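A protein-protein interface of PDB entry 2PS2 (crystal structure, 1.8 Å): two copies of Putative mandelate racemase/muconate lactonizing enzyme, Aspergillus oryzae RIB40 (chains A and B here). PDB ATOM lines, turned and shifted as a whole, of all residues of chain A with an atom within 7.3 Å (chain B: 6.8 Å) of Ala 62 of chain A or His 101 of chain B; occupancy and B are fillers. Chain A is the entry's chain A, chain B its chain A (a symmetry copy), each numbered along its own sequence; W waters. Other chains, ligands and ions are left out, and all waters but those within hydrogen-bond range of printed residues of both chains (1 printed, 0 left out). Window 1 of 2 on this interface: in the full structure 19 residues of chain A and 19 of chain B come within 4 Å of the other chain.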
ATOM      1  N   GLY A  57     -33.204  -5.847  -7.464  1.00  0.00           N
ATOM      2  CA  GLY A  57     -31.848  -5.573  -7.027  1.00  0.00           C
ATOM      3  C   GLY A  57     -31.670  -6.121  -5.624  1.00  0.00           C
ATOM      4  O   GLY A  57     -32.398  -7.027  -5.216  1.00  0.00           O
ATOM      5  N   SER A  58     -30.711  -5.581  -4.880  1.00  0.00           N
ATOM      6  CA  SER A  58     -30.464  -6.035  -3.514  1.00  0.00           C
ATOM      7  C   SER A  58     -30.486  -4.854  -2.547  1.00  0.00           C
ATOM      8  O   SER A  58     -30.070  -4.972  -1.392  1.00  0.00           O
ATOM      9  CB  SER A  58     -29.116  -6.753  -3.434  1.00  0.00           C
ATOM     10  OG  SER A  58     -28.072  -5.947  -3.955  1.00  0.00           O
ATOM     11  N   ASN A  59     -30.997  -3.724  -3.029  1.00  0.00           N
ATOM     12  CA  ASN A  59     -31.074  -2.493  -2.248  1.00  0.00           C
ATOM     13  C   ASN A  59     -32.491  -2.128  -1.803  1.00  0.00           C
ATOM     14  O   ASN A  59     -32.673  -1.283  -0.928  1.00  0.00           O
ATOM     15  CB  ASN A  59     -30.490  -1.336  -3.063  1.00  0.00           C
ATOM     16  CG  ASN A  59     -31.144  -1.195  -4.435  1.00  0.00           C
ATOM     17  OD1 ASN A  59     -30.848  -0.258  -5.183  1.00  0.00           O
ATOM     18  ND2 ASN A  59     -32.034  -2.127  -4.771  1.00  0.00           N
ATOM     19  N   TYR A  60     -33.492  -2.760  -2.407  1.00  0.00           N
ATOM     20  CA  TYR A  60     -34.888  -2.485  -2.070  1.00  0.00           C
ATOM     21  C   TYR A  60     -35.213  -2.954  -0.647  1.00  0.00           C
ATOM     22  O   TYR A  60     -35.601  -2.164   0.220  1.00  0.00           O
ATOM     23  CB  TYR A  60     -35.799  -3.181  -3.087  1.00  0.00           C
ATOM     24  CG  TYR A  60     -37.275  -2.985  -2.839  1.00  0.00           C
ATOM     25  CD1 TYR A  60     -37.822  -1.704  -2.744  1.00  0.00           C
ATOM     26  CD2 TYR A  60     -38.124  -4.080  -2.683  1.00  0.00           C
ATOM     27  CE1 TYR A  60     -39.182  -1.519  -2.498  1.00  0.00           C
ATOM     28  CE2 TYR A  60     -39.486  -3.906  -2.435  1.00  0.00           C
ATOM     29  CZ  TYR A  60     -40.006  -2.624  -2.343  1.00  0.00           C
ATOM     30  OH  TYR A  60     -41.343  -2.449  -2.087  1.00  0.00           O
ATOM     31  N   ILE A  61     -35.056  -4.252  -0.427  1.00  0.00           N
ATOM     32  CA  ILE A  61     -35.295  -4.866   0.872  1.00  0.00           C
ATOM     33  C   ILE A  61     -34.172  -5.878   1.044  1.00  0.00           C
ATOM     34  O   ILE A  61     -33.340  -6.029   0.150  1.00  0.00           O
ATOM     35  CB  ILE A  61     -36.647  -5.595   0.913  1.00  0.00           C
ATOM     36  CG1 ILE A  61     -36.724  -6.594  -0.244  1.00  0.00           C
ATOM     37  CG2 ILE A  61     -37.790  -4.586   0.848  1.00  0.00           C
ATOM     38  CD1 ILE A  61     -38.017  -7.372  -0.300  1.00  0.00           C
ATOM     39  N   ALA A  62     -34.148  -6.564   2.182  1.00  0.00           N
ATOM     40  CA  ALA A  62     -33.113  -7.557   2.456  1.00  0.00           C
ATOM     41  C   ALA A  62     -33.329  -8.790   1.582  1.00  0.00           C
ATOM     42  O   ALA A  62     -33.708  -9.856   2.065  1.00  0.00           O
ATOM     43  CB  ALA A  62     -33.138  -7.940   3.937  1.00  0.00           C
ATOM     44  N   SER A  63     -33.071  -8.633   0.290  1.00  0.00           N
ATOM     45  CA  SER A  63     -33.268  -9.711  -0.667  1.00  0.00           C
ATOM     46  C   SER A  63     -32.385  -9.529  -1.892  1.00  0.00           C
ATOM     47  O   SER A  63     -32.188  -8.410  -2.358  1.00  0.00           O
ATOM     48  CB  SER A  63     -34.740  -9.730  -1.101  1.00  0.00           C
ATOM     49  OG  SER A  63     -34.964 -10.613  -2.185  1.00  0.00           O
ATOM     50  N   HIS A  64     -31.841 -10.633  -2.398  1.00  0.00           N
ATOM     51  CA  HIS A  64     -31.016 -10.597  -3.599  1.00  0.00           C
ATOM     52  C   HIS A  64     -31.136 -11.930  -4.331  1.00  0.00           C
ATOM     53  O   HIS A  64     -31.405 -12.964  -3.716  1.00  0.00           O
ATOM     54  CB  HIS A  64     -29.549 -10.258  -3.268  1.00  0.00           C
ATOM     55  CG  HIS A  64     -28.845 -11.274  -2.422  1.00  0.00           C
ATOM     56  ND1 HIS A  64     -29.311 -11.677  -1.189  1.00  0.00           N
ATOM     57  CD2 HIS A  64     -27.665 -11.912  -2.604  1.00  0.00           C
ATOM     58  CE1 HIS A  64     -28.447 -12.518  -0.647  1.00  0.00           C
ATOM     59  NE2 HIS A  64     -27.439 -12.677  -1.485  1.00  0.00           N
ATOM     60  N   GLY A  67     -29.455 -14.892  -3.020  1.00  0.00           N
ATOM     61  CA  GLY A  67     -30.080 -15.256  -1.760  1.00  0.00           C
ATOM     62  C   GLY A  67     -31.337 -16.079  -1.952  1.00  0.00           C
ATOM     63  O   GLY A  67     -31.619 -16.986  -1.171  1.00  0.00           O
ATOM     64  N   VAL A  68     -32.104 -15.757  -2.989  1.00  0.00           N
ATOM     65  CA  VAL A  68     -33.328 -16.492  -3.284  1.00  0.00           C
ATOM     66  C   VAL A  68     -32.994 -17.948  -3.593  1.00  0.00           C
ATOM     67  O   VAL A  68     -33.596 -18.866  -3.044  1.00  0.00           O
ATOM     68  CB  VAL A  68     -34.066 -15.880  -4.499  1.00  0.00           C
ATOM     69  CG1 VAL A  68     -35.180 -16.816  -4.963  1.00  0.00           C
ATOM     70  CG2 VAL A  68     -34.643 -14.511  -4.124  1.00  0.00           C
ATOM     71  N   HIS A 101     -36.767 -15.279   4.943  1.00  0.00           N
ATOM     72  CA  HIS A 101     -36.549 -15.594   3.534  1.00  0.00           C
ATOM     73  C   HIS A 101     -37.840 -15.783   2.746  1.00  0.00           C
ATOM     74  O   HIS A 101     -37.993 -16.758   1.998  1.00  0.00           O
ATOM     75  CB  HIS A 101     -35.676 -16.848   3.426  1.00  0.00           C
ATOM     76  CG  HIS A 101     -34.324 -16.689   4.045  1.00  0.00           C
ATOM     77  ND1 HIS A 101     -33.234 -16.213   3.345  1.00  0.00           N
ATOM     78  CD2 HIS A 101     -33.901 -16.873   5.317  1.00  0.00           C
ATOM     79  CE1 HIS A 101     -32.201 -16.110   4.162  1.00  0.00           C
ATOM     80  NE2 HIS A 101     -32.579 -16.504   5.364  1.00  0.00           N
ATOM     81  N   GLU A 102     -38.773 -14.851   2.910  1.00  0.00           N
ATOM     82  CA  GLU A 102     -40.033 -14.936   2.185  1.00  0.00           C
ATOM     83  C   GLU A 102     -39.744 -14.994   0.682  1.00  0.00           C
ATOM     84  O   GLU A 102     -40.437 -15.679  -0.067  1.00  0.00           O
ATOM     85  CB  GLU A 102     -40.912 -13.718   2.492  1.00  0.00           C
ATOM     86  CG  GLU A 102     -41.609 -13.736   3.865  1.00  0.00           C
ATOM     87  CD  GLU A 102     -40.655 -13.561   5.039  1.00  0.00           C
ATOM     88  OE1 GLU A 102     -39.636 -12.860   4.882  1.00  0.00           O
ATOM     89  OE2 GLU A 102     -40.937 -14.101   6.133  1.00  0.00           O
ATOM     90  N   ASP A 103     -38.712 -14.274   0.255  1.00  0.00           N
ATOM     91  CA  ASP A 103     -38.350 -14.240  -1.155  1.00  0.00           C
ATOM     92  C   ASP A 103     -37.979 -15.613  -1.703  1.00  0.00           C
ATOM     93  O   ASP A 103     -38.314 -15.934  -2.840  1.00  0.00           O
ATOM     94  CB  ASP A 103     -37.221 -13.226  -1.407  1.00  0.00           C
ATOM     95  CG  ASP A 103     -35.984 -13.462  -0.540  1.00  0.00           C
ATOM     96  OD1 ASP A 103     -36.006 -14.317   0.368  1.00  0.00           O
ATOM     97  OD2 ASP A 103     -34.977 -12.760  -0.770  1.00  0.00           O
ATOM     98  N   GLU A 246     -42.123  -1.708   2.012  1.00  0.00           N
ATOM     99  CA  GLU A 246     -40.906  -2.397   2.444  1.00  0.00           C
ATOM    100  C   GLU A 246     -41.009  -3.020   3.836  1.00  0.00           C
ATOM    101  O   GLU A 246     -40.486  -4.110   4.074  1.00  0.00           O
ATOM    102  CB  GLU A 246     -39.701  -1.447   2.409  1.00  0.00           C
ATOM    103  CG  GLU A 246     -39.148  -1.181   1.018  1.00  0.00           C
ATOM    104  CD  GLU A 246     -39.790   0.022   0.352  1.00  0.00           C
ATOM    105  OE1 GLU A 246     -41.032   0.075   0.277  1.00  0.00           O
ATOM    106  OE2 GLU A 246     -39.043   0.919  -0.095  1.00  0.00           O
ATOM    107  N   ALA B  62     -33.118 -15.764  10.915  1.00  0.00           N
ATOM    108  CA  ALA B  62     -33.161 -15.785   9.455  1.00  0.00           C
ATOM    109  C   ALA B  62     -31.743 -15.783   8.892  1.00  0.00           C
ATOM    110  O   ALA B  62     -31.287 -14.795   8.317  1.00  0.00           O
ATOM    111  CB  ALA B  62     -33.944 -14.576   8.940  1.00  0.00           C
ATOM    112  N   GLY B  67     -26.627 -18.872   2.751  1.00  0.00           N
ATOM    113  CA  GLY B  67     -27.015 -17.472   2.700  1.00  0.00           C
ATOM    114  C   GLY B  67     -25.865 -16.540   3.020  1.00  0.00           C
ATOM    115  O   GLY B  67     -25.749 -15.464   2.438  1.00  0.00           O
ATOM    116  N   VAL B  68     -25.017 -16.946   3.959  1.00  0.00           N
ATOM    117  CA  VAL B  68     -23.861 -16.141   4.337  1.00  0.00           C
ATOM    118  C   VAL B  68     -22.932 -15.975   3.137  1.00  0.00           C
ATOM    119  O   VAL B  68     -22.515 -14.869   2.808  1.00  0.00           O
ATOM    120  CB  VAL B  68     -23.072 -16.804   5.491  1.00  0.00           C
ATOM    121  CG1 VAL B  68     -21.729 -16.103   5.681  1.00  0.00           C
ATOM    122  CG2 VAL B  68     -23.892 -16.746   6.785  1.00  0.00           C
ATOM    123  N   ALA B  70     -23.635 -16.490  -0.069  1.00  0.00           N
ATOM    124  CA  ALA B  70     -24.319 -15.837  -1.182  1.00  0.00           C
ATOM    125  C   ALA B  70     -24.285 -14.321  -0.969  1.00  0.00           C
ATOM    126  O   ALA B  70     -24.098 -13.555  -1.916  1.00  0.00           O
ATOM    127  CB  ALA B  70     -25.766 -16.327  -1.272  1.00  0.00           C
ATOM    128  N   GLY B  71     -24.465 -13.900   0.283  1.00  0.00           N
ATOM    129  CA  GLY B  71     -24.441 -12.485   0.613  1.00  0.00           C
ATOM    130  C   GLY B  71     -23.067 -11.889   0.370  1.00  0.00           C
ATOM    131  O   GLY B  71     -22.933 -10.758  -0.095  1.00  0.00           O
ATOM    132  N   MET B  75     -21.860  -8.738  -2.217  1.00  0.00           N
ATOM    133  CA  MET B  75     -21.191  -7.544  -1.697  1.00  0.00           C
ATOM    134  C   MET B  75     -19.702  -7.371  -2.039  1.00  0.00           C
ATOM    135  O   MET B  75     -19.265  -6.275  -2.389  1.00  0.00           O
ATOM    136  CB  MET B  75     -21.335  -7.484  -0.165  1.00  0.00           C
ATOM    137  CG  MET B  75     -22.776  -7.389   0.360  1.00  0.00           C
ATOM    138  SD  MET B  75     -22.861  -7.172   2.179  1.00  0.00           S
ATOM    139  CE  MET B  75     -22.455  -8.832   2.720  1.00  0.00           C
ATOM    140  N   LEU B  98     -26.133  -4.279  -0.178  1.00  0.00           N
ATOM    141  CA  LEU B  98     -27.122  -5.263   0.267  1.00  0.00           C
ATOM    142  C   LEU B  98     -27.717  -4.907   1.634  1.00  0.00           C
ATOM    143  O   LEU B  98     -26.986  -4.720   2.605  1.00  0.00           O
ATOM    144  CB  LEU B  98     -26.456  -6.637   0.346  1.00  0.00           C
ATOM    145  CG  LEU B  98     -27.276  -7.823   0.855  1.00  0.00           C
ATOM    146  CD1 LEU B  98     -28.371  -8.161  -0.145  1.00  0.00           C
ATOM    147  CD2 LEU B  98     -26.349  -9.019   1.061  1.00  0.00           C
ATOM    148  N   LEU B  99     -29.043  -4.830   1.713  1.00  0.00           N
ATOM    149  CA  LEU B  99     -29.709  -4.496   2.969  1.00  0.00           C
ATOM    150  C   LEU B  99     -29.772  -5.712   3.888  1.00  0.00           C
ATOM    151  O   LEU B  99     -29.908  -6.838   3.421  1.00  0.00           O
ATOM    152  CB  LEU B  99     -31.125  -3.984   2.698  1.00  0.00           C
ATOM    153  CG  LEU B  99     -31.248  -2.804   1.728  1.00  0.00           C
ATOM    154  CD1 LEU B  99     -32.698  -2.364   1.653  1.00  0.00           C
ATOM    155  CD2 LEU B  99     -30.360  -1.651   2.185  1.00  0.00           C
ATOM    156  N   GLY B 100     -29.683  -5.481   5.192  1.00  0.00           N
ATOM    157  CA  GLY B 100     -29.729  -6.581   6.142  1.00  0.00           C
ATOM    158  C   GLY B 100     -28.529  -7.507   6.019  1.00  0.00           C
ATOM    159  O   GLY B 100     -27.397  -7.051   5.877  1.00  0.00           O
ATOM    160  N   HIS B 101     -28.776  -8.811   6.095  1.00  0.00           N
ATOM    161  CA  HIS B 101     -27.714  -9.805   5.973  1.00  0.00           C
ATOM    162  C   HIS B 101     -26.512  -9.524   6.868  1.00  0.00           C
ATOM    163  O   HIS B 101     -25.359  -9.572   6.421  1.00  0.00           O
ATOM    164  CB  HIS B 101     -27.272  -9.896   4.510  1.00  0.00           C
ATOM    165  CG  HIS B 101     -28.365 -10.320   3.582  1.00  0.00           C
ATOM    166  ND1 HIS B 101     -28.626 -11.643   3.291  1.00  0.00           N
ATOM    167  CD2 HIS B 101     -29.311  -9.600   2.935  1.00  0.00           C
ATOM    168  CE1 HIS B 101     -29.687 -11.718   2.507  1.00  0.00           C
ATOM    169  NE2 HIS B 101     -30.122 -10.493   2.276  1.00  0.00           N
ATOM    170  N   GLU B 102     -26.779  -9.231   8.137  1.00  0.00           N
ATOM    171  CA  GLU B 102     -25.695  -8.965   9.073  1.00  0.00           C
ATOM    172  C   GLU B 102     -24.749 -10.169   9.101  1.00  0.00           C
ATOM    173  O   GLU B 102     -23.537 -10.016   9.228  1.00  0.00           O
ATOM    174  CB  GLU B 102     -26.250  -8.717  10.480  1.00  0.00           C
ATOM    175  CG  GLU B 102     -26.888  -7.333  10.703  1.00  0.00           C
ATOM    176  CD  GLU B 102     -28.205  -7.138   9.962  1.00  0.00           C
ATOM    177  OE1 GLU B 102     -28.941  -8.128   9.781  1.00  0.00           O
ATOM    178  OE2 GLU B 102     -28.519  -5.987   9.581  1.00  0.00           O
ATOM    179  N   ASP B 103     -25.318 -11.365   8.973  1.00  0.00           N
ATOM    180  CA  ASP B 103     -24.521 -12.583   8.998  1.00  0.00           C
ATOM    181  C   ASP B 103     -23.493 -12.640   7.875  1.00  0.00           C
ATOM    182  O   ASP B 103     -22.379 -13.115   8.081  1.00  0.00           O
ATOM    183  CB  ASP B 103     -25.423 -13.829   8.979  1.00  0.00           C
ATOM    184  CG  ASP B 103     -26.406 -13.853   7.808  1.00  0.00           C
ATOM    185  OD1 ASP B 103     -26.518 -12.860   7.061  1.00  0.00           O
ATOM    186  OD2 ASP B 103     -27.087 -14.887   7.651  1.00  0.00           O
ATOM    187  N   ALA B 104     -23.851 -12.142   6.695  1.00  0.00           N
ATOM    188  CA  ALA B 104     -22.917 -12.140   5.570  1.00  0.00           C
ATOM    189  C   ALA B 104     -21.882 -11.019   5.701  1.00  0.00           C
ATOM    190  O   ALA B 104     -20.743 -11.157   5.250  1.00  0.00           O
ATOM    191  CB  ALA B 104     -23.677 -11.991   4.262  1.00  0.00           C
ATOM    192  N   LYS B 105     -22.276  -9.910   6.318  1.00  0.00           N
ATOM    193  CA  LYS B 105     -21.372  -8.774   6.488  1.00  0.00           C
ATOM    194  C   LYS B 105     -20.322  -8.995   7.577  1.00  0.00           C
ATOM    195  O   LYS B 105     -19.208  -8.479   7.491  1.00  0.00           O
ATOM    196  CB  LYS B 105     -22.179  -7.511   6.811  1.00  0.00           C
ATOM    197  CG  LYS B 105     -23.109  -7.090   5.681  1.00  0.00           C
ATOM    198  CD  LYS B 105     -24.073  -5.972   6.074  1.00  0.00           C
ATOM    199  CE  LYS B 105     -25.030  -5.682   4.917  1.00  0.00           C
ATOM    200  NZ  LYS B 105     -26.103  -4.701   5.275  1.00  0.00           N
ATOM    201  N   THR B 106     -20.677  -9.785   8.580  1.00  0.00           N
ATOM    202  CA  THR B 106     -19.804 -10.041   9.718  1.00  0.00           C
ATOM    203  C   THR B 106     -18.352 -10.435   9.443  1.00  0.00           C
ATOM    204  O   THR B 106     -17.431  -9.754   9.899  1.00  0.00           O
ATOM    205  CB  THR B 106     -20.435 -11.100  10.650  1.00  0.00           C
ATOM    206  OG1 THR B 106     -21.683 -10.598  11.152  1.00  0.00           O
ATOM    207  CG2 THR B 106     -19.509 -11.400  11.829  1.00  0.00           C
ATOM    208  N   SER B 271     -22.062 -12.209  14.908  1.00  0.00           N
ATOM    209  CA  SER B 271     -22.590 -12.411  13.564  1.00  0.00           C
ATOM    210  C   SER B 271     -24.058 -12.046  13.378  1.00  0.00           C
ATOM    211  O   SER B 271     -24.540 -11.984  12.247  1.00  0.00           O
ATOM    212  CB  SER B 271     -22.327 -13.851  13.083  1.00  0.00           C
ATOM    213  OG  SER B 271     -23.082 -14.795  13.815  1.00  0.00           O
ATOM    214  N   GLY B 274     -23.685  -8.014  13.070  1.00  0.00           N
ATOM    215  CA  GLY B 274     -23.128  -7.582  11.801  1.00  0.00           C
ATOM    216  C   GLY B 274     -21.625  -7.365  11.823  1.00  0.00           C
ATOM    217  O   GLY B 274     -21.052  -6.865  10.846  1.00  0.00           O
HETATM  218  O   HOH W   1     -28.070 -14.503   1.325  1.00  0.00           O
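The backbone carbonyl oxygen (O) of Ser 58 of chain A is in hydrogen-bond range of the backbone NH (N) of Leu 99 of chain B (3.3 Å).
A ring nitrogen (NE2) of His 64 of chain A is in hydrogen-bond range of the backbone carbonyl oxygen (O) of Ala 70 of chain B, at 3.5 Å.
OH of Tyr 60 of chain A lies within hydrogen-bond range of OE1 of Glu 246 of chain A (3.5 Å).
The backbone NH (N) of Gly 67 of chain A sits at hydrogen-bond distance from a ring nitrogen (NE2) of His 64 of chain A (3.4 Å).
The backbone carbonyl oxygen (O) of Leu 98 of chain B is in hydrogen-bond range of the side-chain amino group (NZ) of Lys 105 of chain B.
Among the printed residues, pairs that only touch across the chains: Ser 58 of chain A with Leu 98 of chain B, Asn 59 of chain A with Leu 99 of chain B, Tyr 60 of chain A with Leu 99 of chain B, Ile 61 of chain A with Leu 99 of chain B, Ala 62 of chain A with Leu 99 of chain B, Ala 62 of chain A with His 101 of chain B, His 64 of chain A with Gly 71 of chain B, His 64 of chain A with Leu 98 of chain B, His 64 of chain A with His 101 of chain B and His 101 of chain A with Ala 62 of chain B.
Ala 62 of chain A touches two residues of chain B.
Of the printed residues of chain A, His 101 of chain B touches Ala 62 and His 64.
Of the printed residues of chain B, Ile 61 of chain A touches Leu 99.
Of the printed residues of chain A, Leu 99 of chain B touches Ser 58 (3.3 Å), Asn 59 (2.8 Å), Tyr 60 (3.2 Å), Ile 61 (3.7 Å) and Ala 62 (3.4 Å).
Of the printed residues of chain B, Tyr 60 of chain A touches Leu 99.
Met 75 of chain B touches none of the printed residues of chain A.
The nearest printed residue of chain A that does not touch His 101 of chain B is Ser 63 of chain A (4.01 Å).
The nearest printed residue of chain B that does not touch Asn 59 of chain A is Leu 98 of chain B (5.3 Å).
Printed residues of chain A that touch a printed residue of chain B: Ser 58, Asn 59, Tyr 60, Ile 61, Ala 62, His 64 and His 101.
Hydrophobic or aromatic side chains of chain A that line the printed part of chain B: Ala 62, His 64 and His 101.
Hydrophobic or aromatic side chains of chain B that line the printed part of chain A: Leu 98, Leu 99 and His 101.
Among the printed residues, 12 pairs touch across the chains.
Among the printed residues, no Asp or Glu carboxylate lies within 4 Å of a Lys or Arg side-chain nitrogen of the other chain.
Ala 62 of chain A touches His 101 of chain B, and with the chains exchanged His 101 of chain A touches Ala 62 of chain B.
Positions printed for both chains: 62, 67, 68, 101, 102 and 103.
Of the 12 pairs that touch across the chains among the printed residues, 2 have their exchanged pair printed and touching as well.
Water W1 lies within hydrogen-bond range of the backbone carbonyl oxygen of Gly 67 of chain B and a ring nitrogen (NE2) of His 64 of chain A.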
